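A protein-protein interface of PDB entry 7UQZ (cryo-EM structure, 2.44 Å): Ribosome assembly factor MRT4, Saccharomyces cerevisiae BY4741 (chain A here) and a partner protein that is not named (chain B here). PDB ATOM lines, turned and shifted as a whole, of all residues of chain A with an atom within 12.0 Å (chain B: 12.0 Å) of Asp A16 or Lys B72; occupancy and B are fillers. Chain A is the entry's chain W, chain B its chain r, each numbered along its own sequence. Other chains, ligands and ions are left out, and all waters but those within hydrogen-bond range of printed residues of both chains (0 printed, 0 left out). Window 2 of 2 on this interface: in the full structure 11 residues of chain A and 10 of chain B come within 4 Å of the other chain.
O of Ala A13 is in hydrogen-bond range of NZ of Lys B72 (3.1 Å). The side-chain carboxylate (OD1) of Asp A16 lies within salt-bridge range of the side-chain amino group (NZ) of Lys B72, at 3.2 Å. The backbone carbonyl oxygen (O) of Ala A13 sits at hydrogen-bond distance from a ring nitrogen (NE2) of His B68 (2.9 Å).
Of the printed residues of chain B, Val A10 touches Ile B65 (3.9 Å). Of the printed residues of chain B, Leu A12 touches Lys B64 (3.8 Å), Ile B65 (3.6 Å) and His B68 (3.5 Å). Ala A13 touches just these residues of chain B: His B68 (2.9 Å) and Lys B72 (3.1 Å). No residue of chain B comes within 4 Å of Thr A15. Asp A16 touches just one residue of chain B: Lys B72 (3.2 Å). No residue of chain B comes within 4 Å of Lys A17. No residue of chain B comes within 4 Å of Lys A18. Gly A19 touches none of the printed residues of chain B. Glu A21 touches none of the printed residues of chain B. Of the printed residues of chain A, Lys B64 touches Leu A12. Of the printed residues of chain A, Ile B65 touches Val A10 (3.9 Å) and Leu A12 (3.6 Å). Lys B72 touches three residues of chain A. No residue of chain A comes within 4 Å of Val B73. The nearest residue of chain A that does not touch Lys B72 is Thr A15 (4.9 Å).
Val A10 touches Ile B65. Leu A12 touches Lys B64. Ile B65 touches Leu A12. His B68 touches Leu A12 (CD2 to CD2, 3.5 Å). Lys B72 touches Gln A14.
Hydrophobic or aromatic side chains of chain B that line the printed part of chain A: Ile B65 and His B68. Among the printed residues, Asp or Glu carboxylates within 4 Å of a Lys or Arg side-chain nitrogen of the other chain: Asp A16 with Lys B72.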
ATOM      1  N   LEU A   9       5.769  27.966   3.113  1.00  0.00           N
ATOM      2  CA  LEU A   9       6.550  29.171   2.878  1.00  0.00           C
ATOM      3  C   LEU A   9       6.727  29.397   1.382  1.00  0.00           C
ATOM      4  O   LEU A   9       6.992  28.461   0.623  1.00  0.00           O
ATOM      5  CB  LEU A   9       7.915  29.068   3.558  1.00  0.00           C
ATOM      6  CG  LEU A   9       7.919  28.959   5.083  1.00  0.00           C
ATOM      7  CD1 LEU A   9       9.327  28.702   5.601  1.00  0.00           C
ATOM      8  CD2 LEU A   9       7.334  30.215   5.708  1.00  0.00           C
ATOM      9  N   VAL A  10       6.577  30.648   0.959  1.00  0.00           N
ATOM     10  CA  VAL A  10       6.699  31.030  -0.443  1.00  0.00           C
ATOM     11  C   VAL A  10       7.959  31.865  -0.604  1.00  0.00           C
ATOM     12  O   VAL A  10       8.154  32.853   0.116  1.00  0.00           O
ATOM     13  CB  VAL A  10       5.461  31.800  -0.931  1.00  0.00           C
ATOM     14  CG1 VAL A  10       5.541  32.038  -2.431  1.00  0.00           C
ATOM     15  CG2 VAL A  10       4.192  31.046  -0.570  1.00  0.00           C
ATOM     16  N   THR A  11       8.814  31.467  -1.540  1.00  0.00           N
ATOM     17  CA  THR A  11      10.049  32.176  -1.841  1.00  0.00           C
ATOM     18  C   THR A  11      10.058  32.572  -3.308  1.00  0.00           C
ATOM     19  O   THR A  11       9.652  31.791  -4.174  1.00  0.00           O
ATOM     20  CB  THR A  11      11.275  31.316  -1.529  1.00  0.00           C
ATOM     21  OG1 THR A  11      11.121  30.033  -2.148  1.00  0.00           O
ATOM     22  CG2 THR A  11      11.435  31.137  -0.029  1.00  0.00           C
ATOM     23  N   LEU A  12      10.520  33.788  -3.582  1.00  0.00           N
ATOM     24  CA  LEU A  12      10.559  34.329  -4.938  1.00  0.00           C
ATOM     25  C   LEU A  12      12.004  34.283  -5.422  1.00  0.00           C
ATOM     26  O   LEU A  12      12.753  35.251  -5.298  1.00  0.00           O
ATOM     27  CB  LEU A  12       9.987  35.740  -4.968  1.00  0.00           C
ATOM     28  CG  LEU A  12       8.538  35.833  -4.491  1.00  0.00           C
ATOM     29  CD1 LEU A  12       8.014  37.255  -4.594  1.00  0.00           C
ATOM     30  CD2 LEU A  12       7.673  34.883  -5.291  1.00  0.00           C
ATOM     31  N   ALA A  13      12.393  33.142  -5.982  1.00  0.00           N
ATOM     32  CA  ALA A  13      13.740  32.907  -6.470  1.00  0.00           C
ATOM     33  C   ALA A  13      13.721  32.743  -7.990  1.00  0.00           C
ATOM     34  O   ALA A  13      12.690  32.922  -8.644  1.00  0.00           O
ATOM     35  CB  ALA A  13      14.347  31.691  -5.772  1.00  0.00           C
ATOM     36  N   GLN A  14      14.881  32.402  -8.552  1.00  0.00           N
ATOM     37  CA  GLN A  14      15.052  32.324  -9.997  1.00  0.00           C
ATOM     38  C   GLN A  14      15.084  30.902 -10.538  1.00  0.00           C
ATOM     39  O   GLN A  14      14.886  30.714 -11.744  1.00  0.00           O
ATOM     40  CB  GLN A  14      16.346  33.036 -10.412  1.00  0.00           C
ATOM     41  CG  GLN A  14      16.382  34.510 -10.060  1.00  0.00           C
ATOM     42  CD  GLN A  14      15.384  35.318 -10.856  1.00  0.00           C
ATOM     43  OE1 GLN A  14      15.186  35.080 -12.047  1.00  0.00           O
ATOM     44  NE2 GLN A  14      14.744  36.278 -10.202  1.00  0.00           N
ATOM     45  N   THR A  15      15.327  29.905  -9.695  1.00  0.00           N
ATOM     46  CA  THR A  15      15.531  28.531 -10.136  1.00  0.00           C
ATOM     47  C   THR A  15      14.293  27.700  -9.830  1.00  0.00           C
ATOM     48  O   THR A  15      13.768  27.747  -8.713  1.00  0.00           O
ATOM     49  CB  THR A  15      16.760  27.918  -9.460  1.00  0.00           C
ATOM     50  OG1 THR A  15      17.884  28.789  -9.627  1.00  0.00           O
ATOM     51  CG2 THR A  15      17.087  26.566 -10.069  1.00  0.00           C
ATOM     52  N   ASP A  16      13.830  26.948 -10.822  1.00  0.00           N
ATOM     53  CA  ASP A  16      12.684  26.066 -10.673  1.00  0.00           C
ATOM     54  C   ASP A  16      13.137  24.634 -10.418  1.00  0.00           C
ATOM     55  O   ASP A  16      14.291  24.269 -10.655  1.00  0.00           O
ATOM     56  CB  ASP A  16      11.793  26.116 -11.916  1.00  0.00           C
ATOM     57  CG  ASP A  16      11.152  27.473 -12.119  1.00  0.00           C
ATOM     58  OD1 ASP A  16      11.450  28.395 -11.331  1.00  0.00           O
ATOM     59  OD2 ASP A  16      10.349  27.618 -13.063  1.00  0.00           O
ATOM     60  N   LYS A  17      12.206  23.823  -9.926  1.00  0.00           N
ATOM     61  CA  LYS A  17      12.495  22.421  -9.666  1.00  0.00           C
ATOM     62  C   LYS A  17      12.599  21.639 -10.970  1.00  0.00           C
ATOM     63  O   LYS A  17      11.941  21.948 -11.966  1.00  0.00           O
ATOM     64  CB  LYS A  17      11.415  21.805  -8.778  1.00  0.00           C
ATOM     65  CG  LYS A  17      11.458  22.269  -7.337  1.00  0.00           C
ATOM     66  CD  LYS A  17      10.449  21.520  -6.484  1.00  0.00           C
ATOM     67  CE  LYS A  17      10.491  21.992  -5.042  1.00  0.00           C
ATOM     68  NZ  LYS A  17       9.474  21.303  -4.202  1.00  0.00           N
ATOM     69  N   LYS A  18      13.442  20.613 -10.953  1.00  0.00           N
ATOM     70  CA  LYS A  18      13.601  19.740 -12.104  1.00  0.00           C
ATOM     71  C   LYS A  18      12.508  18.678 -12.117  1.00  0.00           C
ATOM     72  O   LYS A  18      12.113  18.147 -11.074  1.00  0.00           O
ATOM     73  CB  LYS A  18      14.982  19.081 -12.094  1.00  0.00           C
ATOM     74  CG  LYS A  18      16.066  19.874 -12.817  1.00  0.00           C
ATOM     75  CD  LYS A  18      16.426  21.159 -12.087  1.00  0.00           C
ATOM     76  CE  LYS A  18      17.347  22.031 -12.922  1.00  0.00           C
ATOM     77  NZ  LYS A  18      17.602  23.347 -12.278  1.00  0.00           N
ATOM     78  N   GLY A  19      12.016  18.373 -13.314  1.00  0.00           N
ATOM     79  CA  GLY A  19      10.935  17.417 -13.458  1.00  0.00           C
ATOM     80  C   GLY A  19      11.406  16.034 -13.852  1.00  0.00           C
ATOM     81  O   GLY A  19      12.538  15.645 -13.550  1.00  0.00           O
ATOM     82  N   ARG A  20      10.541  15.274 -14.525  1.00  0.00           N
ATOM     83  CA  ARG A  20      10.940  13.959 -15.009  1.00  0.00           C
ATOM     84  C   ARG A  20      11.836  14.053 -16.236  1.00  0.00           C
ATOM     85  O   ARG A  20      12.532  13.082 -16.557  1.00  0.00           O
ATOM     86  CB  ARG A  20       9.698  13.120 -15.321  1.00  0.00           C
ATOM     87  CG  ARG A  20       9.964  11.626 -15.431  1.00  0.00           C
ATOM     88  CD  ARG A  20       8.736  10.873 -15.904  1.00  0.00           C
ATOM     89  NE  ARG A  20       9.028   9.464 -16.134  1.00  0.00           N
ATOM     90  CZ  ARG A  20       9.002   8.532 -15.192  1.00  0.00           C
ATOM     91  NH1 ARG A  20       8.699   8.827 -13.938  1.00  0.00           N
ATOM     92  NH2 ARG A  20       9.290   7.275 -15.513  1.00  0.00           N
ATOM     93  N   GLU A  21      11.835  15.200 -16.923  1.00  0.00           N
ATOM     94  CA  GLU A  21      12.642  15.349 -18.129  1.00  0.00           C
ATOM     95  C   GLU A  21      14.132  15.276 -17.818  1.00  0.00           C
ATOM     96  O   GLU A  21      14.904  14.717 -18.603  1.00  0.00           O
ATOM     97  CB  GLU A  21      12.296  16.659 -18.840  1.00  0.00           C
ATOM     98  CG  GLU A  21      12.244  17.889 -17.945  1.00  0.00           C
ATOM     99  CD  GLU A  21      10.842  18.201 -17.448  1.00  0.00           C
ATOM    100  OE1 GLU A  21       9.978  17.298 -17.480  1.00  0.00           O
ATOM    101  OE2 GLU A  21      10.601  19.353 -17.027  1.00  0.00           O
ATOM    102  N   ASN A  22      14.555  15.830 -16.679  1.00  0.00           N
ATOM    103  CA  ASN A  22      15.963  15.752 -16.297  1.00  0.00           C
ATOM    104  C   ASN A  22      16.384  14.311 -16.028  1.00  0.00           C
ATOM    105  O   ASN A  22      17.464  13.882 -16.457  1.00  0.00           O
ATOM    106  CB  ASN A  22      16.222  16.631 -15.075  1.00  0.00           C
ATOM    107  CG  ASN A  22      17.696  16.904 -14.853  1.00  0.00           C
ATOM    108  OD1 ASN A  22      18.307  17.685 -15.580  1.00  0.00           O
ATOM    109  ND2 ASN A  22      18.270  16.271 -13.839  1.00  0.00           N
ATOM    110  N   LYS A  23      15.537  13.547 -15.333  1.00  0.00           N
ATOM    111  CA  LYS A  23      15.844  12.143 -15.077  1.00  0.00           C
ATOM    112  C   LYS A  23      15.879  11.341 -16.371  1.00  0.00           C
ATOM    113  O   LYS A  23      16.733  10.465 -16.544  1.00  0.00           O
ATOM    114  CB  LYS A  23      14.826  11.552 -14.103  1.00  0.00           C
ATOM    115  CG  LYS A  23      14.882  12.149 -12.708  1.00  0.00           C
ATOM    116  CD  LYS A  23      13.961  11.408 -11.753  1.00  0.00           C
ATOM    117  CE  LYS A  23      12.519  11.472 -12.220  1.00  0.00           C
ATOM    118  NZ  LYS A  23      11.607  10.731 -11.306  1.00  0.00           N
ATOM    119  N   ARG A  25      16.663  12.555 -19.316  1.00  0.00           N
ATOM    120  CA  ARG A  25      17.892  12.956 -19.996  1.00  0.00           C
ATOM    121  C   ARG A  25      19.103  12.231 -19.423  1.00  0.00           C
ATOM    122  O   ARG A  25      19.974  11.776 -20.174  1.00  0.00           O
ATOM    123  CB  ARG A  25      18.079  14.469 -19.893  1.00  0.00           C
ATOM    124  CG  ARG A  25      19.331  14.984 -20.581  1.00  0.00           C
ATOM    125  CD  ARG A  25      19.600  16.436 -20.230  1.00  0.00           C
ATOM    126  NE  ARG A  25      19.831  16.616 -18.801  1.00  0.00           N
ATOM    127  CZ  ARG A  25      21.003  16.453 -18.204  1.00  0.00           C
ATOM    128  NH1 ARG A  25      22.082  16.104 -18.885  1.00  0.00           N
ATOM    129  NH2 ARG A  25      21.095  16.640 -16.891  1.00  0.00           N
ATOM    130  N   LYS B  63      -0.638  40.170  -5.954  1.00  0.00           N
ATOM    131  CA  LYS B  63      -0.035  41.025  -6.973  1.00  0.00           C
ATOM    132  C   LYS B  63       1.482  40.870  -7.006  1.00  0.00           C
ATOM    133  O   LYS B  63       2.086  40.868  -8.083  1.00  0.00           O
ATOM    134  CB  LYS B  63      -0.420  42.484  -6.733  1.00  0.00           C
ATOM    135  CG  LYS B  63      -1.835  42.827  -7.158  1.00  0.00           C
ATOM    136  CD  LYS B  63      -2.163  44.276  -6.844  1.00  0.00           C
ATOM    137  CE  LYS B  63      -3.588  44.615  -7.241  1.00  0.00           C
ATOM    138  NZ  LYS B  63      -3.975  45.978  -6.787  1.00  0.00           N
ATOM    139  N   LYS B  64       2.113  40.741  -5.836  1.00  0.00           N
ATOM    140  CA  LYS B  64       3.559  40.529  -5.792  1.00  0.00           C
ATOM    141  C   LYS B  64       3.952  39.203  -6.437  1.00  0.00           C
ATOM    142  O   LYS B  64       4.932  39.136  -7.194  1.00  0.00           O
ATOM    143  CB  LYS B  64       4.051  40.591  -4.346  1.00  0.00           C
ATOM    144  CG  LYS B  64       5.453  40.051  -4.148  1.00  0.00           C
ATOM    145  CD  LYS B  64       5.838  40.027  -2.681  1.00  0.00           C
ATOM    146  CE  LYS B  64       5.946  41.432  -2.120  1.00  0.00           C
ATOM    147  NZ  LYS B  64       6.384  41.421  -0.698  1.00  0.00           N
ATOM    148  N   ILE B  65       3.199  38.138  -6.148  1.00  0.00           N
ATOM    149  CA  ILE B  65       3.481  36.835  -6.753  1.00  0.00           C
ATOM    150  C   ILE B  65       3.315  36.904  -8.266  1.00  0.00           C
ATOM    151  O   ILE B  65       4.135  36.365  -9.023  1.00  0.00           O
ATOM    152  CB  ILE B  65       2.582  35.745  -6.136  1.00  0.00           C
ATOM    153  CG1 ILE B  65       2.809  35.632  -4.628  1.00  0.00           C
ATOM    154  CG2 ILE B  65       2.828  34.401  -6.800  1.00  0.00           C
ATOM    155  CD1 ILE B  65       4.212  35.272  -4.240  1.00  0.00           C
ATOM    156  N   LYS B  66       2.253  37.571  -8.729  1.00  0.00           N
ATOM    157  CA  LYS B  66       2.028  37.720 -10.164  1.00  0.00           C
ATOM    158  C   LYS B  66       3.153  38.508 -10.825  1.00  0.00           C
ATOM    159  O   LYS B  66       3.600  38.162 -11.924  1.00  0.00           O
ATOM    160  CB  LYS B  66       0.681  38.397 -10.410  1.00  0.00           C
ATOM    161  CG  LYS B  66       0.297  38.531 -11.870  1.00  0.00           C
ATOM    162  CD  LYS B  66       0.076  37.169 -12.509  1.00  0.00           C
ATOM    163  CE  LYS B  66      -0.410  37.308 -13.944  1.00  0.00           C
ATOM    164  NZ  LYS B  66      -0.497  35.987 -14.622  1.00  0.00           N
ATOM    165  N   ALA B  67       3.622  39.572 -10.167  1.00  0.00           N
ATOM    166  CA  ALA B  67       4.720  40.361 -10.714  1.00  0.00           C
ATOM    167  C   ALA B  67       5.998  39.539 -10.813  1.00  0.00           C
ATOM    168  O   ALA B  67       6.715  39.615 -11.818  1.00  0.00           O
ATOM    169  CB  ALA B  67       4.949  41.609  -9.862  1.00  0.00           C
ATOM    170  N   HIS B  68       6.299  38.742  -9.782  1.00  0.00           N
ATOM    171  CA  HIS B  68       7.494  37.902  -9.833  1.00  0.00           C
ATOM    172  C   HIS B  68       7.396  36.852 -10.934  1.00  0.00           C
ATOM    173  O   HIS B  68       8.376  36.595 -11.645  1.00  0.00           O
ATOM    174  CB  HIS B  68       7.735  37.226  -8.486  1.00  0.00           C
ATOM    175  CG  HIS B  68       8.914  36.304  -8.483  1.00  0.00           C
ATOM    176  ND1 HIS B  68      10.214  36.760  -8.455  1.00  0.00           N
ATOM    177  CD2 HIS B  68       8.990  34.953  -8.522  1.00  0.00           C
ATOM    178  CE1 HIS B  68      11.040  35.730  -8.467  1.00  0.00           C
ATOM    179  NE2 HIS B  68      10.323  34.622  -8.509  1.00  0.00           N
ATOM    180  N   GLU B  69       6.225  36.226 -11.086  1.00  0.00           N
ATOM    181  CA  GLU B  69       6.059  35.226 -12.139  1.00  0.00           C
ATOM    182  C   GLU B  69       6.178  35.852 -13.525  1.00  0.00           C
ATOM    183  O   GLU B  69       6.807  35.273 -14.419  1.00  0.00           O
ATOM    184  CB  GLU B  69       4.716  34.511 -11.987  1.00  0.00           C
ATOM    185  CG  GLU B  69       4.646  33.562 -10.800  1.00  0.00           C
ATOM    186  CD  GLU B  69       5.519  32.335 -10.975  1.00  0.00           C
ATOM    187  OE1 GLU B  69       5.840  31.987 -12.131  1.00  0.00           O
ATOM    188  OE2 GLU B  69       5.885  31.713  -9.954  1.00  0.00           O
ATOM    189  N   GLN B  70       5.588  37.034 -13.718  1.00  0.00           N
ATOM    190  CA  GLN B  70       5.710  37.726 -14.998  1.00  0.00           C
ATOM    191  C   GLN B  70       7.157  38.106 -15.285  1.00  0.00           C
ATOM    192  O   GLN B  70       7.619  38.006 -16.427  1.00  0.00           O
ATOM    193  CB  GLN B  70       4.815  38.964 -15.009  1.00  0.00           C
ATOM    194  CG  GLN B  70       4.852  39.751 -16.308  1.00  0.00           C
ATOM    195  CD  GLN B  70       4.027  41.022 -16.243  1.00  0.00           C
ATOM    196  OE1 GLN B  70       3.515  41.390 -15.186  1.00  0.00           O
ATOM    197  NE2 GLN B  70       3.894  41.699 -17.377  1.00  0.00           N
ATOM    198  N   SER B  71       7.887  38.552 -14.258  1.00  0.00           N
ATOM    199  CA  SER B  71       9.294  38.895 -14.440  1.00  0.00           C
ATOM    200  C   SER B  71      10.123  37.670 -14.804  1.00  0.00           C
ATOM    201  O   SER B  71      11.011  37.745 -15.661  1.00  0.00           O
ATOM    202  CB  SER B  71       9.837  39.551 -13.171  1.00  0.00           C
ATOM    203  OG  SER B  71      11.236  39.748 -13.256  1.00  0.00           O
ATOM    204  N   LYS B  72       9.852  36.533 -14.161  1.00  0.00           N
ATOM    205  CA  LYS B  72      10.629  35.328 -14.424  1.00  0.00           C
ATOM    206  C   LYS B  72      10.240  34.646 -15.731  1.00  0.00           C
ATOM    207  O   LYS B  72      11.033  33.856 -16.257  1.00  0.00           O
ATOM    208  CB  LYS B  72      10.490  34.349 -13.256  1.00  0.00           C
ATOM    209  CG  LYS B  72      11.655  33.385 -13.127  1.00  0.00           C
ATOM    210  CD  LYS B  72      11.715  32.750 -11.747  1.00  0.00           C
ATOM    211  CE  LYS B  72      10.462  31.958 -11.437  1.00  0.00           C
ATOM    212  NZ  LYS B  72      10.583  31.243 -10.138  1.00  0.00           N
ATOM    213  N   VAL B  73       9.045  34.922 -16.259  1.00  0.00           N
ATOM    214  CA  VAL B  73       8.676  34.405 -17.576  1.00  0.00           C
ATOM    215  C   VAL B  73       9.615  34.959 -18.643  1.00  0.00           C
ATOM    216  O   VAL B  73      10.109  34.224 -19.506  1.00  0.00           O
ATOM    217  CB  VAL B  73       7.202  34.728 -17.888  1.00  0.00           C
ATOM    218  CG1 VAL B  73       6.948  34.738 -19.389  1.00  0.00           C
ATOM    219  CG2 VAL B  73       6.287  33.719 -17.211  1.00  0.00           C
ATOM    220  N   LYS B  74       9.892  36.258 -18.583  1.00  0.00           N
ATOM    221  CA  LYS B  74      10.844  36.875 -19.499  1.00  0.00           C
ATOM    222  C   LYS B  74      12.252  36.856 -18.916  1.00  0.00           C
ATOM    223  O   LYS B  74      12.671  37.802 -18.250  1.00  0.00           O
ATOM    224  CB  LYS B  74      10.429  38.312 -19.823  1.00  0.00           C
ATOM    225  CG  LYS B  74       9.213  38.420 -20.723  1.00  0.00           C
ATOM    226  CD  LYS B  74       8.996  39.852 -21.185  1.00  0.00           C
ATOM    227  CE  LYS B  74       7.883  39.936 -22.213  1.00  0.00           C
ATOM    228  NZ  LYS B  74       7.698  41.323 -22.725  1.00  0.00           N
